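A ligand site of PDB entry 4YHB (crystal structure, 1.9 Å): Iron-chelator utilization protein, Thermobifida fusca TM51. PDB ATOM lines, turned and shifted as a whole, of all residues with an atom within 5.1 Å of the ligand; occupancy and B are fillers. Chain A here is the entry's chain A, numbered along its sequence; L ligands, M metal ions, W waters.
An oxygen (O13) of the ligand sits close to the backbone nitrogen of Pro 112 (3.4 Å).
Merely in contact with the ligand: His 53 (3.5 Å), Tyr 89 (3.3 Å), Phe 105 (3.8 Å), Gly 111 (3.3 Å), Thr 150 (3.3 Å), Pro 153 (3.6 Å), Pro 201 (3.98 Å), Tyr 255 (3.3 Å), Trp 256 (3.5 Å), Arg 258 (3.4 Å) and His 265 (3.5 Å).
Hydrophobic or aromatic side chains that line the ligand: His 53, Tyr 89, Val 106, His 108, Pro 112, Pro 153, Pro 201, Tyr 255, Trp 256 and His 265.
26 residues have an atom within 4 Å of the ligand: His 53, Arg 87, Asp 88, Tyr 89, Thr 90, Asp 104, Phe 105, Val 106, His 108, Asn 110, Gly 111, Pro 112, Gly 113, Gly 114, Thr 150, Pro 153, Pro 201, Tyr 255, Trp 256, Arg 257, Arg 258, Gly 259, Val 260, Ser 261, Asn 262 and His 265.
NH2 of Arg 87 sits at hydrogen-bond distance from OG of Ser 261 (3.4 Å).
ND1 of His 108 is in hydrogen-bond range of N of Asn 110 (3.1 Å).
A ring nitrogen (ND1) of His 265 lies within hydrogen-bond range of the side-chain carboxylate (OD1) of Asp 253 (3.1 Å).
The backbone carbonyl oxygen (O) of Asp 88 is in hydrogen-bond range of an oxygen (O9) of the ligand (2.7 Å).
The backbone NH (N) of Asn 262 is in hydrogen-bond range of an oxygen (O2) of the ligand (2.7 Å).
O of Arg 257 sits at hydrogen-bond distance from O6 of the ligand (2.7 Å).
The guanidinium group (NE) of Arg 87 lies within salt-bridge range of an oxygen (O13) of the ligand, at 2.7 Å.
An oxygen (O14) of the ligand sits at hydrogen-bond distance from a ring nitrogen (NE2) of His 108 (2.7 Å).
The side-chain hydroxyl (OG) of Ser 261 is in hydrogen-bond range of an oxygen (O1) of the ligand (2.8 Å).
A nitrogen (N7) of the ligand sits at hydrogen-bond distance from the backbone carbonyl oxygen of Asp 104 (2.9 Å).
An oxygen (O7) of the ligand sits at hydrogen-bond distance from the backbone NH (N) of Val 106 (2.9 Å).
The backbone NH (N) of Gly 114 is in hydrogen-bond range of an oxygen (O14) of the ligand, at 2.9 Å.
An oxygen (O13) of the ligand sits at hydrogen-bond distance from the backbone NH of Gly 113 (3.0 Å).
The backbone NH of Thr 90 sits at hydrogen-bond distance from an oxygen (O8) of the ligand, at 3.0 Å.
The side-chain hydroxyl (OG1) of Thr 90 lies within hydrogen-bond range of a nitrogen (N8) of the ligand (3.0 Å).
OD1 of Asn 110 sits close to N5 of the ligand, at 3.4 Å.
The backbone carbonyl oxygen of Val 260 lies close to an oxygen (O6) of the ligand (3.3 Å).
An oxygen (O6) of the ligand sits at hydrogen-bond distance from the backbone NH (N) of Gly 259 (3.3 Å).
Water W5 bridges O1 of the ligand (2.6 Å) and OG of Ser 261 (3.1 Å).
Water W2 bridges a nitrogen (N4) of the ligand (2.7 Å) and the side-chain carboxylate (OE2) of Glu 149 (2.8 Å).
Water W9 bridges O5 of the ligand (2.7 Å) and N of Gly 259 (3.4 Å).
Water W6 lies within hydrogen-bond range of N of Asp 104, O of Thr 90 and O8 of the ligand.
Water W4 lies within hydrogen-bond range of the backbone carbonyl oxygen (O) of Tyr 255, the backbone carbonyl oxygen (O) of Leu 263 and an oxygen (O9) of the ligand.
Water W10 lies within hydrogen-bond range of OD1 of Asn 262 (2.7 Å), N of Asp 88 (2.8 Å) and O9 of the ligand (3.3 Å).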
ATOM      1  N   HIS A  53     -21.435   9.173  23.102  1.00  0.00           N
ATOM      2  CA  HIS A  53     -20.368   9.183  22.104  1.00  0.00           C
ATOM      3  C   HIS A  53     -19.162   8.384  22.564  1.00  0.00           C
ATOM      4  O   HIS A  53     -18.873   8.259  23.752  1.00  0.00           O
ATOM      5  CB  HIS A  53     -19.945  10.619  21.766  1.00  0.00           C
ATOM      6  CG  HIS A  53     -19.605  11.440  22.971  1.00  0.00           C
ATOM      7  ND1 HIS A  53     -20.572  12.016  23.769  1.00  0.00           N
ATOM      8  CD2 HIS A  53     -18.413  11.776  23.524  1.00  0.00           C
ATOM      9  CE1 HIS A  53     -19.991  12.682  24.750  1.00  0.00           C
ATOM     10  NE2 HIS A  53     -18.679  12.541  24.624  1.00  0.00           N
ATOM     11  N   ARG A  87     -10.687  10.481  18.155  1.00  0.00           N
ATOM     12  CA  ARG A  87     -11.657  11.527  17.871  1.00  0.00           C
ATOM     13  C   ARG A  87     -13.013  11.108  18.402  1.00  0.00           C
ATOM     14  O   ARG A  87     -13.331   9.920  18.411  1.00  0.00           O
ATOM     15  CB  ARG A  87     -11.774  11.803  16.358  1.00  0.00           C
ATOM     16  CG  ARG A  87     -10.467  12.064  15.602  1.00  0.00           C
ATOM     17  CD  ARG A  87      -9.919  13.419  15.926  1.00  0.00           C
ATOM     18  NE  ARG A  87      -8.805  13.814  15.067  1.00  0.00           N
ATOM     19  CZ  ARG A  87      -7.517  13.774  15.435  1.00  0.00           C
ATOM     20  NH1 ARG A  87      -7.190  13.332  16.638  1.00  0.00           N
ATOM     21  NH2 ARG A  87      -6.580  14.172  14.593  1.00  0.00           N
ATOM     22  N   ASP A  88     -13.826  12.084  18.812  1.00  0.00           N
ATOM     23  CA  ASP A  88     -15.179  11.849  19.318  1.00  0.00           C
ATOM     24  C   ASP A  88     -16.166  11.623  18.183  1.00  0.00           C
ATOM     25  O   ASP A  88     -16.248  12.454  17.268  1.00  0.00           O
ATOM     26  CB  ASP A  88     -15.673  13.041  20.134  1.00  0.00           C
ATOM     27  CG  ASP A  88     -15.108  13.079  21.524  1.00  0.00           C
ATOM     28  OD1 ASP A  88     -14.119  12.369  21.806  1.00  0.00           O
ATOM     29  OD2 ASP A  88     -15.645  13.843  22.340  1.00  0.00           O
ATOM     30  N   TYR A  89     -16.952  10.545  18.263  1.00  0.00           N
ATOM     31  CA  TYR A  89     -18.053  10.303  17.327  1.00  0.00           C
ATOM     32  C   TYR A  89     -19.264   9.807  18.105  1.00  0.00           C
ATOM     33  O   TYR A  89     -19.145   9.065  19.080  1.00  0.00           O
ATOM     34  CB  TYR A  89     -17.649   9.279  16.239  1.00  0.00           C
ATOM     35  CG  TYR A  89     -16.770   9.877  15.161  1.00  0.00           C
ATOM     36  CD1 TYR A  89     -15.386   9.843  15.277  1.00  0.00           C
ATOM     37  CD2 TYR A  89     -17.319  10.522  14.049  1.00  0.00           C
ATOM     38  CE1 TYR A  89     -14.565  10.399  14.314  1.00  0.00           C
ATOM     39  CE2 TYR A  89     -16.508  11.103  13.068  1.00  0.00           C
ATOM     40  CZ  TYR A  89     -15.126  11.031  13.224  1.00  0.00           C
ATOM     41  OH  TYR A  89     -14.285  11.579  12.285  1.00  0.00           O
ATOM     42  N   THR A  90     -20.444  10.189  17.633  1.00  0.00           N
ATOM     43  CA  THR A  90     -21.687   9.812  18.274  1.00  0.00           C
ATOM     44  C   THR A  90     -22.072   8.351  18.036  1.00  0.00           C
ATOM     45  O   THR A  90     -21.817   7.799  16.963  1.00  0.00           O
ATOM     46  CB  THR A  90     -22.835  10.716  17.771  1.00  0.00           C
ATOM     47  OG1 THR A  90     -22.534  12.083  18.099  1.00  0.00           O
ATOM     48  CG2 THR A  90     -24.193  10.324  18.389  1.00  0.00           C
ATOM     49  N   ILE A 103     -22.125   4.242  13.451  1.00  0.00           N
ATOM     50  CA  ILE A 103     -21.532   5.566  13.521  1.00  0.00           C
ATOM     51  C   ILE A 103     -21.710   6.295  12.194  1.00  0.00           C
ATOM     52  O   ILE A 103     -21.397   5.739  11.131  1.00  0.00           O
ATOM     53  CB  ILE A 103     -20.023   5.515  13.818  1.00  0.00           C
ATOM     54  CG1 ILE A 103     -19.704   4.580  14.983  1.00  0.00           C
ATOM     55  CG2 ILE A 103     -19.464   6.951  13.997  1.00  0.00           C
ATOM     56  CD1 ILE A 103     -19.837   5.187  16.330  1.00  0.00           C
ATOM     57  N   ASP A 104     -22.197   7.531  12.261  1.00  0.00           N
ATOM     58  CA  ASP A 104     -22.276   8.387  11.086  1.00  0.00           C
ATOM     59  C   ASP A 104     -21.066   9.339  11.009  1.00  0.00           C
ATOM     60  O   ASP A 104     -20.882  10.173  11.900  1.00  0.00           O
ATOM     61  CB  ASP A 104     -23.577   9.218  11.114  1.00  0.00           C
ATOM     62  CG  ASP A 104     -24.784   8.417  10.705  1.00  0.00           C
ATOM     63  OD1 ASP A 104     -24.623   7.217  10.419  1.00  0.00           O
ATOM     64  OD2 ASP A 104     -25.897   8.974  10.647  1.00  0.00           O
ATOM     65  N   PHE A 105     -20.273   9.221   9.938  1.00  0.00           N
ATOM     66  CA  PHE A 105     -19.082  10.052   9.756  1.00  0.00           C
ATOM     67  C   PHE A 105     -19.322  11.151   8.726  1.00  0.00           C
ATOM     68  O   PHE A 105     -19.775  10.862   7.617  1.00  0.00           O
ATOM     69  CB  PHE A 105     -17.896   9.235   9.237  1.00  0.00           C
ATOM     70  CG  PHE A 105     -17.362   8.207  10.183  1.00  0.00           C
ATOM     71  CD1 PHE A 105     -18.017   6.996  10.343  1.00  0.00           C
ATOM     72  CD2 PHE A 105     -16.157   8.410  10.844  1.00  0.00           C
ATOM     73  CE1 PHE A 105     -17.495   6.019  11.213  1.00  0.00           C
ATOM     74  CE2 PHE A 105     -15.638   7.447  11.712  1.00  0.00           C
ATOM     75  CZ  PHE A 105     -16.309   6.250  11.890  1.00  0.00           C
ATOM     76  N   VAL A 106     -18.953  12.385   9.057  1.00  0.00           N
ATOM     77  CA  VAL A 106     -18.827  13.394   8.005  1.00  0.00           C
ATOM     78  C   VAL A 106     -17.612  13.053   7.158  1.00  0.00           C
ATOM     79  O   VAL A 106     -16.537  12.788   7.698  1.00  0.00           O
ATOM     80  CB  VAL A 106     -18.666  14.823   8.547  1.00  0.00           C
ATOM     81  CG1 VAL A 106     -18.382  15.808   7.365  1.00  0.00           C
ATOM     82  CG2 VAL A 106     -19.900  15.256   9.312  1.00  0.00           C
ATOM     83  N   HIS A 108     -14.878  14.448   4.987  1.00  0.00           N
ATOM     84  CA  HIS A 108     -14.208  15.700   4.652  1.00  0.00           C
ATOM     85  C   HIS A 108     -12.702  15.419   4.546  1.00  0.00           C
ATOM     86  O   HIS A 108     -12.223  14.353   4.975  1.00  0.00           O
ATOM     87  CB  HIS A 108     -14.493  16.788   5.706  1.00  0.00           C
ATOM     88  CG  HIS A 108     -13.881  16.492   7.043  1.00  0.00           C
ATOM     89  ND1 HIS A 108     -12.667  17.026   7.453  1.00  0.00           N
ATOM     90  CD2 HIS A 108     -14.281  15.685   8.052  1.00  0.00           C
ATOM     91  CE1 HIS A 108     -12.369  16.573   8.662  1.00  0.00           C
ATOM     92  NE2 HIS A 108     -13.332  15.754   9.050  1.00  0.00           N
ATOM     93  N   ASN A 110     -10.107  17.413   5.737  1.00  0.00           N
ATOM     94  CA  ASN A 110      -9.246  18.245   6.566  1.00  0.00           C
ATOM     95  C   ASN A 110      -8.553  17.514   7.720  1.00  0.00           C
ATOM     96  O   ASN A 110      -7.674  18.081   8.361  1.00  0.00           O
ATOM     97  CB  ASN A 110     -10.047  19.418   7.114  1.00  0.00           C
ATOM     98  CG  ASN A 110     -10.738  20.193   6.003  1.00  0.00           C
ATOM     99  OD1 ASN A 110     -11.954  20.385   6.030  1.00  0.00           O
ATOM    100  ND2 ASN A 110      -9.975  20.621   5.026  1.00  0.00           N
ATOM    101  N   GLY A 111      -8.948  16.275   7.991  1.00  0.00           N
ATOM    102  CA  GLY A 111      -8.352  15.526   9.085  1.00  0.00           C
ATOM    103  C   GLY A 111      -8.440  14.032   8.883  1.00  0.00           C
ATOM    104  O   GLY A 111      -9.163  13.562   8.004  1.00  0.00           O
ATOM    105  N   PRO A 112      -7.701  13.263   9.699  1.00  0.00           N
ATOM    106  CA  PRO A 112      -7.612  11.821   9.468  1.00  0.00           C
ATOM    107  C   PRO A 112      -8.939  11.083   9.688  1.00  0.00           C
ATOM    108  O   PRO A 112      -9.150  10.083   9.019  1.00  0.00           O
ATOM    109  CB  PRO A 112      -6.549  11.367  10.482  1.00  0.00           C
ATOM    110  CG  PRO A 112      -6.589  12.376  11.564  1.00  0.00           C
ATOM    111  CD  PRO A 112      -6.914  13.687  10.872  1.00  0.00           C
ATOM    112  N   GLY A 113      -9.806  11.559  10.578  1.00  0.00           N
ATOM    113  CA  GLY A 113     -11.084  10.891  10.773  1.00  0.00           C
ATOM    114  C   GLY A 113     -11.948  11.014   9.519  1.00  0.00           C
ATOM    115  O   GLY A 113     -12.491  10.023   9.023  1.00  0.00           O
ATOM    116  N   GLY A 114     -12.078  12.236   9.029  1.00  0.00           N
ATOM    117  CA  GLY A 114     -12.756  12.495   7.762  1.00  0.00           C
ATOM    118  C   GLY A 114     -12.152  11.712   6.611  1.00  0.00           C
ATOM    119  O   GLY A 114     -12.877  11.156   5.789  1.00  0.00           O
ATOM    120  N   GLU A 149     -23.558  19.322  10.415  1.00  0.00           N
ATOM    121  CA  GLU A 149     -23.483  17.893  10.094  1.00  0.00           C
ATOM    122  C   GLU A 149     -22.769  17.036  11.161  1.00  0.00           C
ATOM    123  O   GLU A 149     -23.028  15.829  11.260  1.00  0.00           O
ATOM    124  CB  GLU A 149     -22.809  17.681   8.719  1.00  0.00           C
ATOM    125  CG  GLU A 149     -21.464  18.399   8.543  1.00  0.00           C
ATOM    126  CD  GLU A 149     -21.613  19.760   7.846  1.00  0.00           C
ATOM    127  OE1 GLU A 149     -22.493  20.543   8.253  1.00  0.00           O
ATOM    128  OE2 GLU A 149     -20.842  20.043   6.905  1.00  0.00           O
ATOM    129  N   THR A 150     -21.902  17.627  11.970  1.00  0.00           N
ATOM    130  CA  THR A 150     -21.203  16.836  13.012  1.00  0.00           C
ATOM    131  C   THR A 150     -22.125  16.458  14.151  1.00  0.00           C
ATOM    132  O   THR A 150     -21.909  15.446  14.833  1.00  0.00           O
ATOM    133  CB  THR A 150     -20.000  17.581  13.619  1.00  0.00           C
ATOM    134  OG1 THR A 150     -20.454  18.777  14.289  1.00  0.00           O
ATOM    135  CG2 THR A 150     -18.982  17.942  12.556  1.00  0.00           C
ATOM    136  N   PRO A 153     -25.965  13.472  13.657  1.00  0.00           N
ATOM    137  CA  PRO A 153     -26.247  12.113  14.158  1.00  0.00           C
ATOM    138  C   PRO A 153     -26.962  12.075  15.502  1.00  0.00           C
ATOM    139  O   PRO A 153     -27.932  11.321  15.664  1.00  0.00           O
ATOM    140  CB  PRO A 153     -24.860  11.492  14.268  1.00  0.00           C
ATOM    141  CG  PRO A 153     -24.074  12.180  13.166  1.00  0.00           C
ATOM    142  CD  PRO A 153     -24.575  13.603  13.191  1.00  0.00           C
ATOM    143  N   PRO A 201     -17.810  24.850   5.731  1.00  0.00           N
ATOM    144  CA  PRO A 201     -18.288  24.457   7.065  1.00  0.00           C
ATOM    145  C   PRO A 201     -17.754  25.398   8.135  1.00  0.00           C
ATOM    146  O   PRO A 201     -16.574  25.735   8.101  1.00  0.00           O
ATOM    147  CB  PRO A 201     -17.714  23.037   7.258  1.00  0.00           C
ATOM    148  CG  PRO A 201     -17.478  22.531   5.898  1.00  0.00           C
ATOM    149  CD  PRO A 201     -17.174  23.734   5.024  1.00  0.00           C
ATOM    150  N   ASP A 253     -23.382  22.474  22.783  1.00  0.00           N
ATOM    151  CA  ASP A 253     -22.166  21.658  22.844  1.00  0.00           C
ATOM    152  C   ASP A 253     -21.377  21.826  21.560  1.00  0.00           C
ATOM    153  O   ASP A 253     -21.833  21.439  20.473  1.00  0.00           O
ATOM    154  CB  ASP A 253     -22.540  20.185  23.080  1.00  0.00           C
ATOM    155  CG  ASP A 253     -21.380  19.366  23.691  1.00  0.00           C
ATOM    156  OD1 ASP A 253     -20.247  19.869  23.746  1.00  0.00           O
ATOM    157  OD2 ASP A 253     -21.618  18.211  24.109  1.00  0.00           O
ATOM    158  N   GLY A 254     -20.200  22.431  21.669  1.00  0.00           N
ATOM    159  CA  GLY A 254     -19.304  22.575  20.544  1.00  0.00           C
ATOM    160  C   GLY A 254     -18.611  21.266  20.210  1.00  0.00           C
ATOM    161  O   GLY A 254     -17.814  20.771  21.000  1.00  0.00           O
ATOM    162  N   TYR A 255     -18.890  20.732  19.013  1.00  0.00           N
ATOM    163  CA  TYR A 255     -18.369  19.418  18.597  1.00  0.00           C
ATOM    164  C   TYR A 255     -17.027  19.506  17.858  1.00  0.00           C
ATOM    165  O   TYR A 255     -16.258  18.550  17.812  1.00  0.00           O
ATOM    166  CB  TYR A 255     -19.400  18.703  17.721  1.00  0.00           C
ATOM    167  CG  TYR A 255     -20.446  17.941  18.519  1.00  0.00           C
ATOM    168  CD1 TYR A 255     -20.608  18.155  19.883  1.00  0.00           C
ATOM    169  CD2 TYR A 255     -21.229  16.974  17.913  1.00  0.00           C
ATOM    170  CE1 TYR A 255     -21.545  17.443  20.615  1.00  0.00           C
ATOM    171  CE2 TYR A 255     -22.185  16.253  18.647  1.00  0.00           C
ATOM    172  CZ  TYR A 255     -22.337  16.502  19.992  1.00  0.00           C
ATOM    173  OH  TYR A 255     -23.268  15.796  20.713  1.00  0.00           O
ATOM    174  N   TRP A 256     -16.758  20.665  17.297  1.00  0.00           N
ATOM    175  CA  TRP A 256     -15.532  20.903  16.576  1.00  0.00           C
ATOM    176  C   TRP A 256     -15.349  22.412  16.440  1.00  0.00           C
ATOM    177  O   TRP A 256     -16.248  23.188  16.772  1.00  0.00           O
ATOM    178  CB  TRP A 256     -15.569  20.249  15.194  1.00  0.00           C
ATOM    179  CG  TRP A 256     -16.486  20.933  14.200  1.00  0.00           C
ATOM    180  CD1 TRP A 256     -17.846  20.929  14.191  1.00  0.00           C
ATOM    181  CD2 TRP A 256     -16.076  21.700  13.065  1.00  0.00           C
ATOM    182  NE1 TRP A 256     -18.328  21.654  13.106  1.00  0.00           N
ATOM    183  CE2 TRP A 256     -17.258  22.132  12.406  1.00  0.00           C
ATOM    184  CE3 TRP A 256     -14.833  22.064  12.533  1.00  0.00           C
ATOM    185  CZ2 TRP A 256     -17.215  22.901  11.243  1.00  0.00           C
ATOM    186  CZ3 TRP A 256     -14.808  22.831  11.378  1.00  0.00           C
ATOM    187  CH2 TRP A 256     -15.984  23.249  10.758  1.00  0.00           C
ATOM    188  N   ARG A 257     -14.183  22.809  15.968  1.00  0.00           N
ATOM    189  CA  ARG A 257     -13.866  24.225  15.796  1.00  0.00           C
ATOM    190  C   ARG A 257     -12.881  24.381  14.651  1.00  0.00           C
ATOM    191  O   ARG A 257     -11.878  23.666  14.606  1.00  0.00           O
ATOM    192  CB  ARG A 257     -13.294  24.816  17.096  1.00  0.00           C
ATOM    193  CG  ARG A 257     -13.062  26.329  17.034  1.00  0.00           C
ATOM    194  CD  ARG A 257     -12.699  26.896  18.400  1.00  0.00           C
ATOM    195  NE  ARG A 257     -12.560  28.342  18.332  1.00  0.00           N
ATOM    196  CZ  ARG A 257     -11.642  29.035  18.993  1.00  0.00           C
ATOM    197  NH1 ARG A 257     -10.764  28.397  19.761  1.00  0.00           N
ATOM    198  NH2 ARG A 257     -11.591  30.352  18.885  1.00  0.00           N
ATOM    199  N   ARG A 258     -13.162  25.300  13.720  1.00  0.00           N
ATOM    200  CA  ARG A 258     -12.255  25.562  12.596  1.00  0.00           C
ATOM    201  C   ARG A 258     -10.860  25.915  13.094  1.00  0.00           C
ATOM    202  O   ARG A 258     -10.714  26.711  14.015  1.00  0.00           O
ATOM    203  CB  ARG A 258     -12.775  26.720  11.724  1.00  0.00           C
ATOM    204  CG  ARG A 258     -14.062  26.421  10.991  1.00  0.00           C
ATOM    205  CD  ARG A 258     -14.529  27.656  10.191  1.00  0.00           C
ATOM    206  NE  ARG A 258     -13.459  28.201   9.370  1.00  0.00           N
ATOM    207  CZ  ARG A 258     -12.863  29.370   9.601  1.00  0.00           C
ATOM    208  NH1 ARG A 258     -13.262  30.117  10.631  1.00  0.00           N
ATOM    209  NH2 ARG A 258     -11.898  29.801   8.811  1.00  0.00           N
ATOM    210  N   GLY A 259      -9.857  25.306  12.466  1.00  0.00           N
ATOM    211  CA  GLY A 259      -8.468  25.546  12.806  1.00  0.00           C
ATOM    212  C   GLY A 259      -7.991  24.777  14.033  1.00  0.00           C
ATOM    213  O   GLY A 259      -6.835  24.902  14.436  1.00  0.00           O
ATOM    214  N   VAL A 260      -8.876  23.979  14.626  1.00  0.00           N
ATOM    215  CA  VAL A 260      -8.515  23.190  15.799  1.00  0.00           C
ATOM    216  C   VAL A 260      -8.640  21.704  15.502  1.00  0.00           C
ATOM    217  O   VAL A 260      -9.666  21.256  14.989  1.00  0.00           O
ATOM    218  CB  VAL A 260      -9.386  23.541  17.009  1.00  0.00           C
ATOM    219  CG1 VAL A 260      -9.016  22.698  18.244  1.00  0.00           C
ATOM    220  CG2 VAL A 260      -9.285  25.041  17.328  1.00  0.00           C
ATOM    221  N   SER A 261      -7.607  20.939  15.802  1.00  0.00           N
ATOM    222  CA  SER A 261      -7.673  19.493  15.613  1.00  0.00           C
ATOM    223  C   SER A 261      -8.067  18.814  16.923  1.00  0.00           C
ATOM    224  O   SER A 261      -7.515  19.118  17.985  1.00  0.00           O
ATOM    225  CB  SER A 261      -6.321  18.973  15.101  1.00  0.00           C
ATOM    226  OG  SER A 261      -6.322  17.557  15.035  1.00  0.00           O
ATOM    227  N   ASN A 262      -9.041  17.897  16.837  1.00  0.00           N
ATOM    228  CA  ASN A 262      -9.487  17.104  17.983  1.00  0.00           C
ATOM    229  C   ASN A 262      -9.876  17.980  19.182  1.00  0.00           C
ATOM    230  O   ASN A 262      -9.333  17.823  20.269  1.00  0.00           O
ATOM    231  CB  ASN A 262      -8.405  16.089  18.397  1.00  0.00           C
ATOM    232  CG  ASN A 262      -8.932  15.032  19.375  1.00  0.00           C
ATOM    233  OD1 ASN A 262     -10.145  14.807  19.466  1.00  0.00           O
ATOM    234  ND2 ASN A 262      -8.035  14.392  20.106  1.00  0.00           N
ATOM    235  N   LEU A 263     -10.813  18.902  18.951  1.00  0.00           N
ATOM    236  CA  LEU A 263     -11.358  19.733  20.016  1.00  0.00           C
ATOM    237  C   LEU A 263     -11.851  18.901  21.196  1.00  0.00           C
ATOM    238  O   LEU A 263     -12.586  17.940  20.994  1.00  0.00           O
ATOM    239  CB  LEU A 263     -12.523  20.585  19.484  1.00  0.00           C
ATOM    240  CG  LEU A 263     -13.246  21.428  20.535  1.00  0.00           C
ATOM    241  CD1 LEU A 263     -12.318  22.549  21.001  1.00  0.00           C
ATOM    242  CD2 LEU A 263     -14.556  22.029  19.979  1.00  0.00           C
ATOM    243  N   HIS A 265     -14.336  18.678  23.985  1.00  0.00           N
ATOM    244  CA  HIS A 265     -15.558  19.389  24.326  1.00  0.00           C
ATOM    245  C   HIS A 265     -15.836  19.381  25.833  1.00  0.00           C
ATOM    246  O   HIS A 265     -16.784  20.012  26.306  1.00  0.00           O
ATOM    247  CB  HIS A 265     -16.741  18.808  23.538  1.00  0.00           C
ATOM    248  CG  HIS A 265     -17.287  17.532  24.102  1.00  0.00           C
ATOM    249  ND1 HIS A 265     -18.633  17.304  24.266  1.00  0.00           N
ATOM    250  CD2 HIS A 265     -16.662  16.422  24.564  1.00  0.00           C
ATOM    251  CE1 HIS A 265     -18.822  16.098  24.769  1.00  0.00           C
ATOM    252  NE2 HIS A 265     -17.637  15.555  24.990  1.00  0.00           N
HETATM  253  P1  LIG L   1      -9.308  16.870  13.008  1.00  0.00           P
HETATM  254  O1  LIG L   1      -7.867  16.341  13.003  1.00  0.00           O
HETATM  255  O2  LIG L   1      -9.909  16.906  14.472  1.00  0.00           O
HETATM  256  O3  LIG L   1      -9.268  18.413  12.541  1.00  0.00           O
HETATM  257  C1  LIG L   1      -8.484  18.794  11.467  1.00  0.00           C
HETATM  258  C2  LIG L   1      -9.089  20.059  10.819  1.00  0.00           C
HETATM  259  O4  LIG L   1     -10.309  19.793  10.185  1.00  0.00           O
HETATM  260  C3  LIG L   1      -9.341  21.139  11.786  1.00  0.00           C
HETATM  261  O5  LIG L   1      -9.009  22.318  11.144  1.00  0.00           O
HETATM  262  C4  LIG L   1     -10.735  21.068  12.034  1.00  0.00           C
HETATM  263  O6  LIG L   1     -11.336  22.326  12.314  1.00  0.00           O
HETATM  264  C5  LIG L   1     -11.295  20.587  10.767  1.00  0.00           C
HETATM  265  N1  LIG L   1     -12.515  19.792  10.883  1.00  0.00           N
HETATM  266  C6  LIG L   1     -12.793  18.870  11.819  1.00  0.00           C
HETATM  267  N2  LIG L   1     -14.002  18.353  11.564  1.00  0.00           N
HETATM  268  C7  LIG L   1     -14.474  18.914  10.434  1.00  0.00           C
HETATM  269  C8  LIG L   1     -15.643  18.776   9.685  1.00  0.00           C
HETATM  270  N3  LIG L   1     -16.641  17.852  10.093  1.00  0.00           N
HETATM  271  N4  LIG L   1     -15.814  19.518   8.576  1.00  0.00           N
HETATM  272  C9  LIG L   1     -14.873  20.398   8.175  1.00  0.00           C
HETATM  273  N5  LIG L   1     -13.740  20.557   8.864  1.00  0.00           N
HETATM  274  C10 LIG L   1     -13.530  19.839  10.000  1.00  0.00           C
HETATM  275  N6  LIG L   1     -18.419  14.121  13.819  1.00  0.00           N
HETATM  276  C11 LIG L   1     -19.020  13.316  12.944  1.00  0.00           C
HETATM  277  O7  LIG L   1     -18.721  13.376  11.755  1.00  0.00           O
HETATM  278  N7  LIG L   1     -19.958  12.432  13.406  1.00  0.00           N
HETATM  279  C12 LIG L   1     -20.284  12.357  14.716  1.00  0.00           C
HETATM  280  O8  LIG L   1     -21.122  11.544  15.065  1.00  0.00           O
HETATM  281  C13 LIG L   1     -19.674  13.194  15.650  1.00  0.00           C
HETATM  282  N8  LIG L   1     -19.967  13.160  17.000  1.00  0.00           N
HETATM  283  C14 LIG L   1     -19.320  13.992  17.861  1.00  0.00           C
HETATM  284  C15 LIG L   1     -19.608  13.961  19.224  1.00  0.00           C
HETATM  285  C16 LIG L   1     -19.019  14.709  20.024  1.00  0.00           C
HETATM  286  C17 LIG L   1     -19.425  14.582  21.504  1.00  0.00           C
HETATM  287  C18 LIG L   1     -18.142  15.547  19.755  1.00  0.00           C
HETATM  288  C19 LIG L   1     -17.469  16.441  20.755  1.00  0.00           C
HETATM  289  C20 LIG L   1     -17.735  15.701  18.453  1.00  0.00           C
HETATM  290  C21 LIG L   1     -18.302  14.907  17.279  1.00  0.00           C
HETATM  291  N9  LIG L   1     -18.050  14.921  15.986  1.00  0.00           N
HETATM  292  C22 LIG L   1     -18.710  14.090  15.146  1.00  0.00           C
HETATM  293  C23 LIG L   1     -17.038  15.864  15.453  1.00  0.00           C
HETATM  294  C24 LIG L   1     -15.686  15.243  15.277  1.00  0.00           C
HETATM  295  O9  LIG L   1     -15.225  14.818  16.497  1.00  0.00           O
HETATM  296  C25 LIG L   1     -14.736  16.321  14.646  1.00  0.00           C
HETATM  297  O10 LIG L   1     -15.325  16.745  13.458  1.00  0.00           O
HETATM  298  C26 LIG L   1     -13.299  15.891  14.490  1.00  0.00           C
HETATM  299  O11 LIG L   1     -12.500  16.990  14.394  1.00  0.00           O
HETATM  300  C27 LIG L   1     -13.046  15.055  13.225  1.00  0.00           C
HETATM  301  O12 LIG L   1     -11.823  14.366  13.256  1.00  0.00           O
HETATM  302  P2  LIG L   1     -10.814  14.694  12.080  1.00  0.00           P
HETATM  303  O13 LIG L   1      -9.588  13.835  12.462  1.00  0.00           O
HETATM  304  O14 LIG L   1     -11.648  14.498  10.791  1.00  0.00           O
HETATM  305  O15 LIG L   1     -10.092  16.080  11.859  1.00  0.00           O
HETATM  306 ZN    ZN M   1     -17.434  13.653  26.020  1.00  0.00          ZN
HETATM  307  O   HOH W   1     -12.616  23.293   8.422  1.00  0.00           O
HETATM  308  O   HOH W   2     -18.133  19.350   7.186  1.00  0.00           O
HETATM  309  O   HOH W   3     -16.536  15.243  11.434  1.00  0.00           O
HETATM  310  O   HOH W   4     -14.066  17.129  18.513  1.00  0.00           O
HETATM  311  O   HOH W   5      -5.442  16.878  12.118  1.00  0.00           O
HETATM  312  O   HOH W   6     -22.506   9.104  14.548  1.00  0.00           O
HETATM  313  O   HOH W   7      -6.203  22.343  10.583  1.00  0.00           O
HETATM  314  O   HOH W   8     -12.537  18.266  16.776  1.00  0.00           O
HETATM  315  O   HOH W   9     -10.298  23.934   9.350  1.00  0.00           O
HETATM  316  O   HOH W  10     -12.788  14.669  18.749  1.00  0.00           O
